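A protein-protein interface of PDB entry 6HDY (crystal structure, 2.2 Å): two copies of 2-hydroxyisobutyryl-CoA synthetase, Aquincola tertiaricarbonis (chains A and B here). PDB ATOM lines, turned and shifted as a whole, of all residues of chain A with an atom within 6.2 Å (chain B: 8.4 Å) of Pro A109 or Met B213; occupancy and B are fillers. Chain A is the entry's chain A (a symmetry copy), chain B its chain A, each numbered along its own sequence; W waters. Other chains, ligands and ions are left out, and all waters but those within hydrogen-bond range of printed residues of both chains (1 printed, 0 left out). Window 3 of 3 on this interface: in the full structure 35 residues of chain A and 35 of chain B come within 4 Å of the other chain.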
ATOM      1  N   GLN A 104     -17.397  16.012  -1.915  1.00  0.00           N
ATOM      2  CA  GLN A 104     -18.483  16.607  -2.700  1.00  0.00           C
ATOM      3  C   GLN A 104     -19.450  17.410  -1.817  1.00  0.00           C
ATOM      4  O   GLN A 104     -19.815  18.529  -2.193  1.00  0.00           O
ATOM      5  CB  GLN A 104     -19.204  15.549  -3.531  1.00  0.00           C
ATOM      6  CG  GLN A 104     -18.326  15.065  -4.676  1.00  0.00           C
ATOM      7  CD  GLN A 104     -19.084  14.482  -5.827  1.00  0.00           C
ATOM      8  OE1 GLN A 104     -20.315  14.360  -5.816  1.00  0.00           O
ATOM      9  NE2 GLN A 104     -18.352  14.120  -6.857  1.00  0.00           N
ATOM     10  N   HIS A 107     -17.264  20.442  -0.787  1.00  0.00           N
ATOM     11  CA  HIS A 107     -16.882  21.246  -1.958  1.00  0.00           C
ATOM     12  C   HIS A 107     -17.792  20.907  -3.147  1.00  0.00           C
ATOM     13  O   HIS A 107     -17.372  20.244  -4.097  1.00  0.00           O
ATOM     14  CB  HIS A 107     -15.378  21.107  -2.260  1.00  0.00           C
ATOM     15  CG  HIS A 107     -14.531  21.342  -1.049  1.00  0.00           C
ATOM     16  ND1 HIS A 107     -14.255  22.625  -0.600  1.00  0.00           N
ATOM     17  CD2 HIS A 107     -14.008  20.448  -0.178  1.00  0.00           C
ATOM     18  CE1 HIS A 107     -13.533  22.469   0.500  1.00  0.00           C
ATOM     19  NE2 HIS A 107     -13.349  21.175   0.787  1.00  0.00           N
ATOM     20  N   PRO A 108     -19.075  21.341  -3.085  1.00  0.00           N
ATOM     21  CA  PRO A 108     -20.004  21.001  -4.162  1.00  0.00           C
ATOM     22  C   PRO A 108     -19.773  21.747  -5.478  1.00  0.00           C
ATOM     23  O   PRO A 108     -19.266  22.858  -5.466  1.00  0.00           O
ATOM     24  CB  PRO A 108     -21.370  21.318  -3.544  1.00  0.00           C
ATOM     25  CG  PRO A 108     -21.115  22.387  -2.575  1.00  0.00           C
ATOM     26  CD  PRO A 108     -19.737  22.166  -2.043  1.00  0.00           C
ATOM     27  N   PRO A 109     -20.159  21.174  -6.632  1.00  0.00           N
ATOM     28  CA  PRO A 109     -20.768  19.852  -6.824  1.00  0.00           C
ATOM     29  C   PRO A 109     -19.817  18.672  -7.026  1.00  0.00           C
ATOM     30  O   PRO A 109     -20.236  17.531  -6.800  1.00  0.00           O
ATOM     31  CB  PRO A 109     -21.642  20.072  -8.056  1.00  0.00           C
ATOM     32  CG  PRO A 109     -20.915  21.116  -8.869  1.00  0.00           C
ATOM     33  CD  PRO A 109     -20.027  21.894  -7.915  1.00  0.00           C
ATOM     34  N   PHE A 110     -18.573  18.910  -7.486  1.00  0.00           N
ATOM     35  CA  PHE A 110     -17.653  17.825  -7.870  1.00  0.00           C
ATOM     36  C   PHE A 110     -16.570  17.424  -6.859  1.00  0.00           C
ATOM     37  O   PHE A 110     -15.838  16.464  -7.112  1.00  0.00           O
ATOM     38  CB  PHE A 110     -17.001  18.157  -9.221  1.00  0.00           C
ATOM     39  CG  PHE A 110     -18.040  18.431 -10.275  1.00  0.00           C
ATOM     40  CD1 PHE A 110     -19.027  17.488 -10.569  1.00  0.00           C
ATOM     41  CD2 PHE A 110     -18.097  19.668 -10.914  1.00  0.00           C
ATOM     42  CE1 PHE A 110     -20.038  17.773 -11.490  1.00  0.00           C
ATOM     43  CE2 PHE A 110     -19.096  19.936 -11.859  1.00  0.00           C
ATOM     44  CZ  PHE A 110     -20.042  18.974 -12.158  1.00  0.00           C
ATOM     45  N   GLY A 111     -16.486  18.119  -5.733  1.00  0.00           N
ATOM     46  CA  GLY A 111     -15.484  17.794  -4.726  1.00  0.00           C
ATOM     47  C   GLY A 111     -14.163  18.511  -4.907  1.00  0.00           C
ATOM     48  O   GLY A 111     -13.925  19.190  -5.917  1.00  0.00           O
ATOM     49  N   ASN A 118     -13.731  24.838 -13.636  1.00  0.00           N
ATOM     50  CA  ASN A 118     -15.152  24.664 -13.937  1.00  0.00           C
ATOM     51  C   ASN A 118     -15.437  24.733 -15.443  1.00  0.00           C
ATOM     52  O   ASN A 118     -16.206  23.932 -15.954  1.00  0.00           O
ATOM     53  CB  ASN A 118     -15.967  25.734 -13.208  1.00  0.00           C
ATOM     54  CG  ASN A 118     -17.220  25.202 -12.562  1.00  0.00           C
ATOM     55  OD1 ASN A 118     -17.246  24.087 -12.007  1.00  0.00           O
ATOM     56  ND2 ASN A 118     -18.283  26.004 -12.609  1.00  0.00           N
ATOM     57  N   VAL A 124     -21.683  15.898 -17.335  1.00  0.00           N
ATOM     58  CA  VAL A 124     -22.114  15.672 -15.959  1.00  0.00           C
ATOM     59  C   VAL A 124     -22.856  14.346 -15.915  1.00  0.00           C
ATOM     60  O   VAL A 124     -23.819  14.153 -16.647  1.00  0.00           O
ATOM     61  CB  VAL A 124     -22.924  16.834 -15.329  1.00  0.00           C
ATOM     62  CG1 VAL A 124     -23.354  16.499 -13.900  1.00  0.00           C
ATOM     63  CG2 VAL A 124     -22.129  18.141 -15.359  1.00  0.00           C
ATOM     64  N   THR A 135     -22.901  10.604  -6.014  1.00  0.00           N
ATOM     65  CA  THR A 135     -21.706  11.358  -6.360  1.00  0.00           C
ATOM     66  C   THR A 135     -21.815  11.813  -7.788  1.00  0.00           C
ATOM     67  O   THR A 135     -22.223  11.044  -8.652  1.00  0.00           O
ATOM     68  CB  THR A 135     -20.417  10.579  -6.078  1.00  0.00           C
ATOM     69  OG1 THR A 135     -20.672   9.202  -6.255  1.00  0.00           O
ATOM     70  CG2 THR A 135     -19.907  10.809  -4.677  1.00  0.00           C
ATOM     71  N   ALA A 136     -21.459  13.064  -8.027  1.00  0.00           N
ATOM     72  CA  ALA A 136     -21.496  13.678  -9.342  1.00  0.00           C
ATOM     73  C   ALA A 136     -20.157  13.544 -10.067  1.00  0.00           C
ATOM     74  O   ALA A 136     -19.099  13.808  -9.497  1.00  0.00           O
ATOM     75  CB  ALA A 136     -21.870  15.151  -9.205  1.00  0.00           C
ATOM     76  N   GLN A 335     -11.238  14.961 -12.004  1.00  0.00           N
ATOM     77  CA  GLN A 335     -11.564  13.950 -10.981  1.00  0.00           C
ATOM     78  C   GLN A 335     -10.626  12.732 -11.051  1.00  0.00           C
ATOM     79  O   GLN A 335     -11.108  11.602 -11.112  1.00  0.00           O
ATOM     80  CB  GLN A 335     -13.054  13.554 -11.023  1.00  0.00           C
ATOM     81  CG  GLN A 335     -13.977  14.741 -10.648  1.00  0.00           C
ATOM     82  CD  GLN A 335     -15.438  14.324 -10.591  1.00  0.00           C
ATOM     83  OE1 GLN A 335     -15.954  13.662 -11.492  1.00  0.00           O
ATOM     84  NE2 GLN A 335     -16.144  14.723  -9.539  1.00  0.00           N
ATOM     85  N   LEU B 165     -24.725  24.900 -17.133  1.00  0.00           N
ATOM     86  CA  LEU B 165     -25.131  23.525 -16.931  1.00  0.00           C
ATOM     87  C   LEU B 165     -26.461  23.323 -17.693  1.00  0.00           C
ATOM     88  O   LEU B 165     -27.459  24.007 -17.411  1.00  0.00           O
ATOM     89  CB  LEU B 165     -25.273  23.199 -15.439  1.00  0.00           C
ATOM     90  CG  LEU B 165     -25.644  21.728 -15.149  1.00  0.00           C
ATOM     91  CD1 LEU B 165     -24.460  20.859 -15.262  1.00  0.00           C
ATOM     92  CD2 LEU B 165     -26.191  21.571 -13.759  1.00  0.00           C
ATOM     93  N   VAL B 166     -26.449  22.411 -18.694  1.00  0.00           N
ATOM     94  CA  VAL B 166     -27.619  22.144 -19.530  1.00  0.00           C
ATOM     95  C   VAL B 166     -28.153  20.766 -19.214  1.00  0.00           C
ATOM     96  O   VAL B 166     -27.477  19.774 -19.493  1.00  0.00           O
ATOM     97  CB  VAL B 166     -27.317  22.305 -21.046  1.00  0.00           C
ATOM     98  CG1 VAL B 166     -28.568  22.017 -21.891  1.00  0.00           C
ATOM     99  CG2 VAL B 166     -26.766  23.692 -21.353  1.00  0.00           C
ATOM    100  N   CYS B 167     -29.362  20.698 -18.635  1.00  0.00           N
ATOM    101  CA  CYS B 167     -29.973  19.416 -18.356  1.00  0.00           C
ATOM    102  C   CYS B 167     -30.741  18.929 -19.568  1.00  0.00           C
ATOM    103  O   CYS B 167     -31.737  19.551 -19.936  1.00  0.00           O
ATOM    104  CB  CYS B 167     -30.866  19.472 -17.123  1.00  0.00           C
ATOM    105  SG  CYS B 167     -31.557  17.864 -16.661  1.00  0.00           S
ATOM    106  N   LYS B 191     -21.790  22.780 -19.805  1.00  0.00           N
ATOM    107  CA  LYS B 191     -21.577  21.553 -19.031  1.00  0.00           C
ATOM    108  C   LYS B 191     -22.795  20.666 -19.402  1.00  0.00           C
ATOM    109  O   LYS B 191     -23.900  20.887 -18.890  1.00  0.00           O
ATOM    110  CB  LYS B 191     -21.561  21.840 -17.519  1.00  0.00           C
ATOM    111  CG  LYS B 191     -20.359  22.606 -17.030  1.00  0.00           C
ATOM    112  CD  LYS B 191     -20.609  23.057 -15.602  1.00  0.00           C
ATOM    113  CE  LYS B 191     -19.472  23.866 -15.039  1.00  0.00           C
ATOM    114  NZ  LYS B 191     -19.161  25.071 -15.860  1.00  0.00           N
ATOM    115  N   PHE B 193     -25.410  17.964 -19.290  1.00  0.00           N
ATOM    116  CA  PHE B 193     -25.926  17.079 -18.246  1.00  0.00           C
ATOM    117  C   PHE B 193     -27.012  16.140 -18.863  1.00  0.00           C
ATOM    118  O   PHE B 193     -28.225  16.408 -18.743  1.00  0.00           O
ATOM    119  CB  PHE B 193     -26.442  17.916 -17.042  1.00  0.00           C
ATOM    120  CG  PHE B 193     -27.109  17.141 -15.930  1.00  0.00           C
ATOM    121  CD1 PHE B 193     -26.678  15.859 -15.593  1.00  0.00           C
ATOM    122  CD2 PHE B 193     -28.128  17.717 -15.175  1.00  0.00           C
ATOM    123  CE1 PHE B 193     -27.298  15.138 -14.564  1.00  0.00           C
ATOM    124  CE2 PHE B 193     -28.728  17.012 -14.119  1.00  0.00           C
ATOM    125  CZ  PHE B 193     -28.316  15.724 -13.822  1.00  0.00           C
ATOM    126  N   LEU B 206     -34.377  13.073 -10.575  1.00  0.00           N
ATOM    127  CA  LEU B 206     -34.066  14.281 -11.334  1.00  0.00           C
ATOM    128  C   LEU B 206     -34.294  15.549 -10.554  1.00  0.00           C
ATOM    129  O   LEU B 206     -33.447  16.427 -10.592  1.00  0.00           O
ATOM    130  CB  LEU B 206     -34.851  14.338 -12.664  1.00  0.00           C
ATOM    131  CG  LEU B 206     -34.536  15.536 -13.620  1.00  0.00           C
ATOM    132  CD1 LEU B 206     -32.994  15.715 -13.837  1.00  0.00           C
ATOM    133  CD2 LEU B 206     -35.206  15.314 -14.977  1.00  0.00           C
ATOM    134  N   VAL B 207     -35.447  15.674  -9.888  1.00  0.00           N
ATOM    135  CA  VAL B 207     -35.781  16.866  -9.108  1.00  0.00           C
ATOM    136  C   VAL B 207     -34.712  17.114  -8.031  1.00  0.00           C
ATOM    137  O   VAL B 207     -34.290  18.262  -7.867  1.00  0.00           O
ATOM    138  CB  VAL B 207     -37.244  16.903  -8.570  1.00  0.00           C
ATOM    139  CG1 VAL B 207     -38.234  16.993  -9.727  1.00  0.00           C
ATOM    140  CG2 VAL B 207     -37.567  15.708  -7.671  1.00  0.00           C
ATOM    141  N   GLN B 208     -34.199  16.034  -7.388  1.00  0.00           N
ATOM    142  CA  GLN B 208     -33.100  16.133  -6.420  1.00  0.00           C
ATOM    143  C   GLN B 208     -31.840  16.648  -7.107  1.00  0.00           C
ATOM    144  O   GLN B 208     -31.203  17.538  -6.552  1.00  0.00           O
ATOM    145  CB  GLN B 208     -32.817  14.787  -5.714  1.00  0.00           C
ATOM    146  CG  GLN B 208     -33.944  14.281  -4.800  1.00  0.00           C
ATOM    147  CD  GLN B 208     -34.278  15.187  -3.613  1.00  0.00           C
ATOM    148  OE1 GLN B 208     -33.506  16.082  -3.195  1.00  0.00           O
ATOM    149  NE2 GLN B 208     -35.459  14.967  -3.041  1.00  0.00           N
ATOM    150  N   TRP B 209     -31.502  16.126  -8.340  1.00  0.00           N
ATOM    151  CA  TRP B 209     -30.339  16.580  -9.103  1.00  0.00           C
ATOM    152  C   TRP B 209     -30.455  18.025  -9.529  1.00  0.00           C
ATOM    153  O   TRP B 209     -29.452  18.723  -9.524  1.00  0.00           O
ATOM    154  CB  TRP B 209     -30.046  15.676 -10.322  1.00  0.00           C
ATOM    155  CG  TRP B 209     -29.289  14.443  -9.952  1.00  0.00           C
ATOM    156  CD1 TRP B 209     -29.813  13.280  -9.469  1.00  0.00           C
ATOM    157  CD2 TRP B 209     -27.874  14.257 -10.000  1.00  0.00           C
ATOM    158  NE1 TRP B 209     -28.814  12.378  -9.219  1.00  0.00           N
ATOM    159  CE2 TRP B 209     -27.608  12.950  -9.531  1.00  0.00           C
ATOM    160  CE3 TRP B 209     -26.798  15.049 -10.434  1.00  0.00           C
ATOM    161  CZ2 TRP B 209     -26.310  12.434  -9.444  1.00  0.00           C
ATOM    162  CZ3 TRP B 209     -25.518  14.522 -10.367  1.00  0.00           C
ATOM    163  CH2 TRP B 209     -25.284  13.244  -9.856  1.00  0.00           C
ATOM    164  N   LEU B 210     -31.665  18.483  -9.902  1.00  0.00           N
ATOM    165  CA  LEU B 210     -31.906  19.875 -10.320  1.00  0.00           C
ATOM    166  C   LEU B 210     -31.791  20.839  -9.127  1.00  0.00           C
ATOM    167  O   LEU B 210     -31.316  21.968  -9.292  1.00  0.00           O
ATOM    168  CB  LEU B 210     -33.283  20.030 -10.980  1.00  0.00           C
ATOM    169  CG  LEU B 210     -33.577  19.155 -12.216  1.00  0.00           C
ATOM    170  CD1 LEU B 210     -35.053  19.164 -12.525  1.00  0.00           C
ATOM    171  CD2 LEU B 210     -32.785  19.595 -13.427  1.00  0.00           C
ATOM    172  N   ASP B 211     -32.234  20.391  -7.933  1.00  0.00           N
ATOM    173  CA  ASP B 211     -32.148  21.160  -6.692  1.00  0.00           C
ATOM    174  C   ASP B 211     -30.683  21.280  -6.266  1.00  0.00           C
ATOM    175  O   ASP B 211     -30.263  22.357  -5.860  1.00  0.00           O
ATOM    176  CB  ASP B 211     -32.976  20.486  -5.583  1.00  0.00           C
ATOM    177  CG  ASP B 211     -33.164  21.343  -4.331  1.00  0.00           C
ATOM    178  OD1 ASP B 211     -34.016  22.263  -4.363  1.00  0.00           O
ATOM    179  OD2 ASP B 211     -32.505  21.053  -3.310  1.00  0.00           O
ATOM    180  N   THR B 212     -29.899  20.183  -6.382  1.00  0.00           N
ATOM    181  CA  THR B 212     -28.475  20.174  -6.033  1.00  0.00           C
ATOM    182  C   THR B 212     -27.625  20.955  -7.053  1.00  0.00           C
ATOM    183  O   THR B 212     -26.887  21.862  -6.660  1.00  0.00           O
ATOM    184  CB  THR B 212     -27.969  18.730  -5.872  1.00  0.00           C
ATOM    185  OG1 THR B 212     -28.794  18.023  -4.939  1.00  0.00           O
ATOM    186  CG2 THR B 212     -26.496  18.662  -5.443  1.00  0.00           C
ATOM    187  N   MET B 213     -27.717  20.584  -8.347  1.00  0.00           N
ATOM    188  CA  MET B 213     -26.915  21.130  -9.455  1.00  0.00           C
ATOM    189  C   MET B 213     -27.284  22.537  -9.883  1.00  0.00           C
ATOM    190  O   MET B 213     -26.411  23.262 -10.337  1.00  0.00           O
ATOM    191  CB  MET B 213     -26.946  20.192 -10.686  1.00  0.00           C
ATOM    192  CG  MET B 213     -26.284  18.842 -10.486  1.00  0.00           C
ATOM    193  SD  MET B 213     -24.486  18.902 -10.225  1.00  0.00           S
ATOM    194  CE  MET B 213     -24.403  17.786  -8.913  1.00  0.00           C
ATOM    195  N   LYS B 214     -28.575  22.915  -9.784  1.00  0.00           N
ATOM    196  CA  LYS B 214     -29.095  24.245 -10.168  1.00  0.00           C
ATOM    197  C   LYS B 214     -28.705  24.630 -11.640  1.00  0.00           C
ATOM    198  O   LYS B 214     -27.937  25.569 -11.856  1.00  0.00           O
ATOM    199  CB  LYS B 214     -28.728  25.345  -9.133  1.00  0.00           C
ATOM    200  CG  LYS B 214     -29.077  24.964  -7.690  1.00  0.00           C
ATOM    201  CD  LYS B 214     -30.036  25.932  -7.037  1.00  0.00           C
ATOM    202  CE  LYS B 214     -30.144  25.721  -5.542  1.00  0.00           C
ATOM    203  NZ  LYS B 214     -31.256  24.798  -5.176  1.00  0.00           N
ATOM    204  N   PRO B 215     -29.247  23.913 -12.665  1.00  0.00           N
ATOM    205  CA  PRO B 215     -28.869  24.211 -14.058  1.00  0.00           C
ATOM    206  C   PRO B 215     -29.387  25.518 -14.621  1.00  0.00           C
ATOM    207  O   PRO B 215     -30.478  25.975 -14.254  1.00  0.00           O
ATOM    208  CB  PRO B 215     -29.463  23.031 -14.832  1.00  0.00           C
ATOM    209  CG  PRO B 215     -30.653  22.648 -14.036  1.00  0.00           C
ATOM    210  CD  PRO B 215     -30.170  22.758 -12.614  1.00  0.00           C
ATOM    211  N   ALA B 216     -28.628  26.090 -15.556  1.00  0.00           N
ATOM    212  CA  ALA B 216     -29.054  27.317 -16.213  1.00  0.00           C
ATOM    213  C   ALA B 216     -30.103  27.012 -17.282  1.00  0.00           C
ATOM    214  O   ALA B 216     -30.930  27.876 -17.570  1.00  0.00           O
ATOM    215  CB  ALA B 216     -27.862  28.031 -16.829  1.00  0.00           C
ATOM    216  N   ASN B 241     -36.634  26.906  -7.353  1.00  0.00           N
ATOM    217  CA  ASN B 241     -35.339  26.852  -6.700  1.00  0.00           C
ATOM    218  C   ASN B 241     -34.352  25.948  -7.441  1.00  0.00           C
ATOM    219  O   ASN B 241     -33.406  25.446  -6.837  1.00  0.00           O
ATOM    220  CB  ASN B 241     -35.490  26.439  -5.214  1.00  0.00           C
ATOM    221  CG  ASN B 241     -34.446  27.012  -4.258  1.00  0.00           C
ATOM    222  OD1 ASN B 241     -33.297  27.316  -4.623  1.00  0.00           O
ATOM    223  ND2 ASN B 241     -34.821  27.137  -2.988  1.00  0.00           N
ATOM    224  N   PHE B 242     -34.550  25.778  -8.765  1.00  0.00           N
ATOM    225  CA  PHE B 242     -33.689  24.942  -9.604  1.00  0.00           C
ATOM    226  C   PHE B 242     -32.642  25.774 -10.359  1.00  0.00           C
ATOM    227  O   PHE B 242     -31.841  25.223 -11.111  1.00  0.00           O
ATOM    228  CB  PHE B 242     -34.550  24.092 -10.554  1.00  0.00           C
ATOM    229  CG  PHE B 242     -35.365  22.984  -9.910  1.00  0.00           C
ATOM    230  CD1 PHE B 242     -35.149  22.612  -8.582  1.00  0.00           C
ATOM    231  CD2 PHE B 242     -36.305  22.272 -10.648  1.00  0.00           C
ATOM    232  CE1 PHE B 242     -35.866  21.557  -8.004  1.00  0.00           C
ATOM    233  CE2 PHE B 242     -37.000  21.194 -10.079  1.00  0.00           C
ATOM    234  CZ  PHE B 242     -36.785  20.853  -8.758  1.00  0.00           C
ATOM    235  N   GLY B 243     -32.664  27.093 -10.137  1.00  0.00           N
ATOM    236  CA  GLY B 243     -31.750  28.065 -10.737  1.00  0.00           C
ATOM    237  C   GLY B 243     -31.866  28.233 -12.237  1.00  0.00           C
ATOM    238  O   GLY B 243     -30.955  28.786 -12.856  1.00  0.00           O
ATOM    239  N   LEU B 244     -32.996  27.768 -12.833  1.00  0.00           N
ATOM    240  CA  LEU B 244     -33.227  27.798 -14.278  1.00  0.00           C
ATOM    241  C   LEU B 244     -33.440  29.173 -14.828  1.00  0.00           C
ATOM    242  O   LEU B 244     -34.245  29.944 -14.286  1.00  0.00           O
ATOM    243  CB  LEU B 244     -34.394  26.873 -14.699  1.00  0.00           C
ATOM    244  CG  LEU B 244     -34.158  25.367 -14.555  1.00  0.00           C
ATOM    245  CD1 LEU B 244     -35.460  24.638 -14.344  1.00  0.00           C
ATOM    246  CD2 LEU B 244     -33.363  24.791 -15.753  1.00  0.00           C
HETATM  247  O   HOH W   1     -17.659  24.011 -18.770  1.00  0.00           O
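O of Asn A118 sits at hydrogen-bond distance from NZ of Lys B191.
O of Leu B165 sits at hydrogen-bond distance from N of Ala B216 (3.0 Å).
N of Val B166 is in hydrogen-bond range of O of Lys B191, 3.0 Å away.
O of Val B166 sits at hydrogen-bond distance from N of Phe B193, at 2.8 Å.
The side-chain amide oxygen (OE1) of Gln A104 sits close to the backbone carbonyl oxygen (O) of Pro A109.
The side-chain amide nitrogen of Gln A104 is in hydrogen-bond range of the backbone carbonyl oxygen of Ala A136 (2.8 Å).
O of Ala A136 lies within hydrogen-bond range of NE2 of Gln A335 (3.1 Å).
Among the printed residues, merely in contact across the chains: Pro A109 with Met B213, Val A124 with Leu B165, Val A124 with Phe B193, Thr A135 with Trp B209, Ala A136 with Trp B209 and Ala A136 with Met B213.
Printed residues of chain B within 4 Å of Asn A118: Lys B191.
Of the printed residues of chain A, Phe B193 touches Val A124 (3.5 Å).
Printed residues of chain B within 4 Å of Thr A135: Trp B209 (3.96 Å).
Leu B206 touches none of the printed residues of chain A.
The nearest residue of chain B that does not touch Pro A109 is Thr B212 (5.7 Å).
Printed residues of chain B that touch a printed residue of chain A: Leu B165, Lys B191, Phe B193, Trp B209 and Met B213.
Hydrophobic or aromatic side chains of chain B that line the printed part of chain A: Leu B165, Phe B193, Trp B209 and Met B213.
Among the printed residues, no Asp or Glu carboxylate lies within 4 Å of a Lys or Arg side-chain nitrogen of the other chain.
No position is printed for both chains.
Water W1 lies within hydrogen-bond range of the backbone carbonyl oxygen (O) of Asn A118 and the side-chain amino group (NZ) of Lys B191.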
